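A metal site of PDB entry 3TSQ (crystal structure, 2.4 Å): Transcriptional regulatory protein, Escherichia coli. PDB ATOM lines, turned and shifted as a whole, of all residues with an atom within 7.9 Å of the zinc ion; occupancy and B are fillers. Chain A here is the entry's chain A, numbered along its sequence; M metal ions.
SG of Cys 23 binds the zinc ion.
The side-chain sulfur (SG) of Cys 42 is bound to the zinc ion (2.4 Å).
The zinc ion is bound by SG of Cys 45 (2.4 Å).
The zinc ion is bound by the side-chain sulfur (SG) of Cys 20 (2.5 Å).
The backbone carbonyl oxygen (O) of Cys 42 is in hydrogen-bond range of the guanidinium group (NH1) of Arg 48 (3.2 Å).
The side-chain sulfur (SG) of Cys 20 lies close to the backbone NH (N) of Ala 22 (3.7 Å).
The guanidinium group (NE) of Arg 83 sits close to the side-chain sulfur (SG) of Cys 42, 3.4 Å away.
NH2 of Arg 83 lies close to SG of Cys 23 (3.4 Å).
The backbone carbonyl oxygen (O) of Cys 45 is in hydrogen-bond range of the guanidinium group (NH1) of Arg 48 (3.0 Å).
The side-chain sulfur (SG) of Cys 42 lies close to the backbone NH (N) of His 44.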
ATOM      1  N   ALA A  17     -18.387  20.943 -15.854  1.00  0.00           N
ATOM      2  CA  ALA A  17     -17.200  21.130 -15.048  1.00  0.00           C
ATOM      3  C   ALA A  17     -15.956  20.754 -15.814  1.00  0.00           C
ATOM      4  O   ALA A  17     -15.913  19.714 -16.456  1.00  0.00           O
ATOM      5  CB  ALA A  17     -17.282  20.354 -13.710  1.00  0.00           C
ATOM      6  N   ALA A  18     -14.921  21.608 -15.715  1.00  0.00           N
ATOM      7  CA  ALA A  18     -13.619  21.331 -16.317  1.00  0.00           C
ATOM      8  C   ALA A  18     -13.131  19.954 -15.863  1.00  0.00           C
ATOM      9  O   ALA A  18     -13.317  19.644 -14.686  1.00  0.00           O
ATOM     10  CB  ALA A  18     -12.647  22.383 -15.864  1.00  0.00           C
ATOM     11  N   THR A  19     -12.498  19.153 -16.747  1.00  0.00           N
ATOM     12  CA  THR A  19     -11.800  17.920 -16.348  1.00  0.00           C
ATOM     13  C   THR A  19     -10.932  18.087 -15.047  1.00  0.00           C
ATOM     14  O   THR A  19     -10.145  19.038 -14.930  1.00  0.00           O
ATOM     15  CB  THR A  19     -10.937  17.444 -17.525  1.00  0.00           C
ATOM     16  OG1 THR A  19     -11.775  17.392 -18.692  1.00  0.00           O
ATOM     17  CG2 THR A  19     -10.272  16.008 -17.271  1.00  0.00           C
ATOM     18  N   CYS A  20     -11.097  17.180 -14.070  1.00  0.00           N
ATOM     19  CA  CYS A  20     -10.414  17.316 -12.760  1.00  0.00           C
ATOM     20  C   CYS A  20      -8.973  16.773 -12.764  1.00  0.00           C
ATOM     21  O   CYS A  20      -8.589  16.040 -13.686  1.00  0.00           O
ATOM     22  CB  CYS A  20     -11.252  16.667 -11.667  1.00  0.00           C
ATOM     23  SG  CYS A  20     -11.175  14.814 -11.654  1.00  0.00           S
ATOM     24  N   PRO A  21      -8.141  17.117 -11.744  1.00  0.00           N
ATOM     25  CA  PRO A  21      -6.759  16.532 -11.758  1.00  0.00           C
ATOM     26  C   PRO A  21      -6.708  15.007 -11.865  1.00  0.00           C
ATOM     27  O   PRO A  21      -5.962  14.474 -12.671  1.00  0.00           O
ATOM     28  CB  PRO A  21      -6.126  17.024 -10.447  1.00  0.00           C
ATOM     29  CG  PRO A  21      -6.909  18.294 -10.125  1.00  0.00           C
ATOM     30  CD  PRO A  21      -8.345  18.004 -10.584  1.00  0.00           C
ATOM     31  N   ALA A  22      -7.516  14.308 -11.092  1.00  0.00           N
ATOM     32  CA  ALA A  22      -7.538  12.824 -11.107  1.00  0.00           C
ATOM     33  C   ALA A  22      -7.899  12.188 -12.484  1.00  0.00           C
ATOM     34  O   ALA A  22      -7.361  11.160 -12.836  1.00  0.00           O
ATOM     35  CB  ALA A  22      -8.440  12.291  -9.993  1.00  0.00           C
ATOM     36  N   CYS A  23      -8.808  12.785 -13.240  1.00  0.00           N
ATOM     37  CA  CYS A  23      -9.132  12.253 -14.552  1.00  0.00           C
ATOM     38  C   CYS A  23      -7.981  12.568 -15.518  1.00  0.00           C
ATOM     39  O   CYS A  23      -7.580  11.722 -16.296  1.00  0.00           O
ATOM     40  CB  CYS A  23     -10.432  12.846 -15.102  1.00  0.00           C
ATOM     41  SG  CYS A  23     -11.914  12.074 -14.404  1.00  0.00           S
ATOM     42  N   LEU A  24      -7.470  13.797 -15.462  1.00  0.00           N
ATOM     43  CA  LEU A  24      -6.274  14.196 -16.190  1.00  0.00           C
ATOM     44  C   LEU A  24      -5.086  13.258 -15.961  1.00  0.00           C
ATOM     45  O   LEU A  24      -4.494  12.766 -16.921  1.00  0.00           O
ATOM     46  CB  LEU A  24      -5.901  15.651 -15.888  1.00  0.00           C
ATOM     47  CG  LEU A  24      -4.931  16.188 -16.947  1.00  0.00           C
ATOM     48  CD1 LEU A  24      -5.651  16.218 -18.306  1.00  0.00           C
ATOM     49  CD2 LEU A  24      -4.283  17.593 -16.601  1.00  0.00           C
ATOM     50  N   GLU A  26      -5.368  10.148 -14.871  1.00  0.00           N
ATOM     51  CA  GLU A  26      -5.710   8.833 -15.426  1.00  0.00           C
ATOM     52  C   GLU A  26      -5.519   8.781 -16.963  1.00  0.00           C
ATOM     53  O   GLU A  26      -5.045   7.781 -17.505  1.00  0.00           O
ATOM     54  CB  GLU A  26      -7.123   8.446 -14.995  1.00  0.00           C
ATOM     55  CG  GLU A  26      -7.707   7.145 -15.551  1.00  0.00           C
ATOM     56  CD  GLU A  26      -9.182   6.934 -15.126  1.00  0.00           C
ATOM     57  OE1 GLU A  26      -9.675   7.664 -14.205  1.00  0.00           O
ATOM     58  OE2 GLU A  26      -9.868   6.072 -15.729  1.00  0.00           O
ATOM     59  N   ILE A  40     -13.005  10.859 -21.088  1.00  0.00           N
ATOM     60  CA  ILE A  40     -12.890  10.580 -19.677  1.00  0.00           C
ATOM     61  C   ILE A  40     -13.632  11.668 -18.840  1.00  0.00           C
ATOM     62  O   ILE A  40     -13.462  12.870 -19.096  1.00  0.00           O
ATOM     63  CB  ILE A  40     -11.401  10.438 -19.290  1.00  0.00           C
ATOM     64  CG1 ILE A  40     -11.213   9.992 -17.834  1.00  0.00           C
ATOM     65  CG2 ILE A  40     -10.623  11.736 -19.549  1.00  0.00           C
ATOM     66  CD1 ILE A  40      -9.738   9.540 -17.559  1.00  0.00           C
ATOM     67  N   ASN A  41     -14.485  11.218 -17.892  1.00  0.00           N
ATOM     68  CA  ASN A  41     -15.097  12.080 -16.856  1.00  0.00           C
ATOM     69  C   ASN A  41     -15.319  11.248 -15.620  1.00  0.00           C
ATOM     70  O   ASN A  41     -15.156  10.037 -15.675  1.00  0.00           O
ATOM     71  CB  ASN A  41     -16.425  12.723 -17.289  1.00  0.00           C
ATOM     72  CG  ASN A  41     -17.443  11.708 -17.794  1.00  0.00           C
ATOM     73  OD1 ASN A  41     -17.532  11.468 -19.000  1.00  0.00           O
ATOM     74  ND2 ASN A  41     -18.224  11.110 -16.884  1.00  0.00           N
ATOM     75  N   CYS A  42     -15.683  11.872 -14.515  1.00  0.00           N
ATOM     76  CA  CYS A  42     -16.008  11.148 -13.314  1.00  0.00           C
ATOM     77  C   CYS A  42     -17.105  11.907 -12.578  1.00  0.00           C
ATOM     78  O   CYS A  42     -17.754  12.788 -13.108  1.00  0.00           O
ATOM     79  CB  CYS A  42     -14.777  10.958 -12.404  1.00  0.00           C
ATOM     80  SG  CYS A  42     -14.251  12.507 -11.550  1.00  0.00           S
ATOM     81  N   THR A  43     -17.295  11.551 -11.324  1.00  0.00           N
ATOM     82  CA  THR A  43     -18.404  12.072 -10.547  1.00  0.00           C
ATOM     83  C   THR A  43     -18.230  13.557 -10.282  1.00  0.00           C
ATOM     84  O   THR A  43     -19.205  14.256 -10.084  1.00  0.00           O
ATOM     85  CB  THR A  43     -18.594  11.257  -9.205  1.00  0.00           C
ATOM     86  OG1 THR A  43     -19.907  11.507  -8.700  1.00  0.00           O
ATOM     87  CG2 THR A  43     -17.561  11.622  -8.145  1.00  0.00           C
ATOM     88  N   HIS A  44     -16.974  14.007 -10.303  1.00  0.00           N
ATOM     89  CA  HIS A  44     -16.592  15.404 -10.045  1.00  0.00           C
ATOM     90  C   HIS A  44     -16.397  16.291 -11.285  1.00  0.00           C
ATOM     91  O   HIS A  44     -16.199  17.468 -11.115  1.00  0.00           O
ATOM     92  CB  HIS A  44     -15.313  15.451  -9.188  1.00  0.00           C
ATOM     93  CG  HIS A  44     -15.469  14.755  -7.885  1.00  0.00           C
ATOM     94  ND1 HIS A  44     -14.785  13.593  -7.565  1.00  0.00           N
ATOM     95  CD2 HIS A  44     -16.330  14.978  -6.858  1.00  0.00           C
ATOM     96  CE1 HIS A  44     -15.162  13.174  -6.368  1.00  0.00           C
ATOM     97  NE2 HIS A  44     -16.102  13.988  -5.925  1.00  0.00           N
ATOM     98  N   CYS A  45     -16.396  15.771 -12.514  1.00  0.00           N
ATOM     99  CA  CYS A  45     -16.077  16.630 -13.640  1.00  0.00           C
ATOM    100  C   CYS A  45     -16.818  16.162 -14.904  1.00  0.00           C
ATOM    101  O   CYS A  45     -17.425  15.090 -14.890  1.00  0.00           O
ATOM    102  CB  CYS A  45     -14.558  16.700 -13.869  1.00  0.00           C
ATOM    103  SG  CYS A  45     -13.917  15.282 -14.757  1.00  0.00           S
ATOM    104  N   GLY A  46     -16.764  16.936 -15.987  1.00  0.00           N
ATOM    105  CA  GLY A  46     -17.377  16.523 -17.228  1.00  0.00           C
ATOM    106  C   GLY A  46     -18.608  17.340 -17.539  1.00  0.00           C
ATOM    107  O   GLY A  46     -18.974  18.221 -16.779  1.00  0.00           O
ATOM    108  N   ARG A  48     -22.527  18.431 -18.132  1.00  0.00           N
ATOM    109  CA  ARG A  48     -23.739  18.149 -17.316  1.00  0.00           C
ATOM    110  C   ARG A  48     -24.975  18.616 -18.069  1.00  0.00           C
ATOM    111  O   ARG A  48     -25.633  17.853 -18.757  1.00  0.00           O
ATOM    112  CB  ARG A  48     -23.653  18.804 -15.898  1.00  0.00           C
ATOM    113  CG  ARG A  48     -22.558  18.263 -14.973  1.00  0.00           C
ATOM    114  CD  ARG A  48     -22.849  16.804 -14.523  1.00  0.00           C
ATOM    115  NE  ARG A  48     -21.795  16.319 -13.612  1.00  0.00           N
ATOM    116  CZ  ARG A  48     -20.750  15.583 -13.982  1.00  0.00           C
ATOM    117  NH1 ARG A  48     -19.852  15.231 -13.094  1.00  0.00           N
ATOM    118  NH2 ARG A  48     -20.590  15.196 -15.252  1.00  0.00           N
ATOM    119  N   ARG A  83     -14.386   6.691  -7.808  1.00  0.00           N
ATOM    120  CA  ARG A  83     -14.504   8.082  -8.265  1.00  0.00           C
ATOM    121  C   ARG A  83     -15.573   8.313  -9.356  1.00  0.00           C
ATOM    122  O   ARG A  83     -16.016   9.457  -9.563  1.00  0.00           O
ATOM    123  CB  ARG A  83     -13.141   8.639  -8.743  1.00  0.00           C
ATOM    124  CG  ARG A  83     -13.127  10.185  -8.807  1.00  0.00           C
ATOM    125  CD  ARG A  83     -11.795  10.785  -9.217  1.00  0.00           C
ATOM    126  NE  ARG A  83     -11.522  10.676 -10.642  1.00  0.00           N
ATOM    127  CZ  ARG A  83     -10.833   9.679 -11.203  1.00  0.00           C
ATOM    128  NH1 ARG A  83     -10.387   8.682 -10.469  1.00  0.00           N
ATOM    129  NH2 ARG A  83     -10.610   9.639 -12.502  1.00  0.00           N
ATOM    130  N   ARG A  84     -15.959   7.228 -10.037  1.00  0.00           N
ATOM    131  CA  ARG A  84     -16.932   7.244 -11.140  1.00  0.00           C
ATOM    132  C   ARG A  84     -18.270   6.614 -10.745  1.00  0.00           C
ATOM    133  O   ARG A  84     -19.076   6.249 -11.623  1.00  0.00           O
ATOM    134  CB  ARG A  84     -16.361   6.536 -12.374  1.00  0.00           C
ATOM    135  CG  ARG A  84     -15.092   7.173 -12.865  1.00  0.00           C
ATOM    136  CD  ARG A  84     -14.238   6.262 -13.693  1.00  0.00           C
ATOM    137  NE  ARG A  84     -12.852   6.263 -13.184  1.00  0.00           N
ATOM    138  CZ  ARG A  84     -12.343   5.342 -12.343  1.00  0.00           C
ATOM    139  NH1 ARG A  84     -13.088   4.323 -11.910  1.00  0.00           N
ATOM    140  NH2 ARG A  84     -11.092   5.438 -11.956  1.00  0.00           N
HETATM  141 ZN    ZN M   1     -12.928  13.770 -13.135  1.00  0.00          ZN
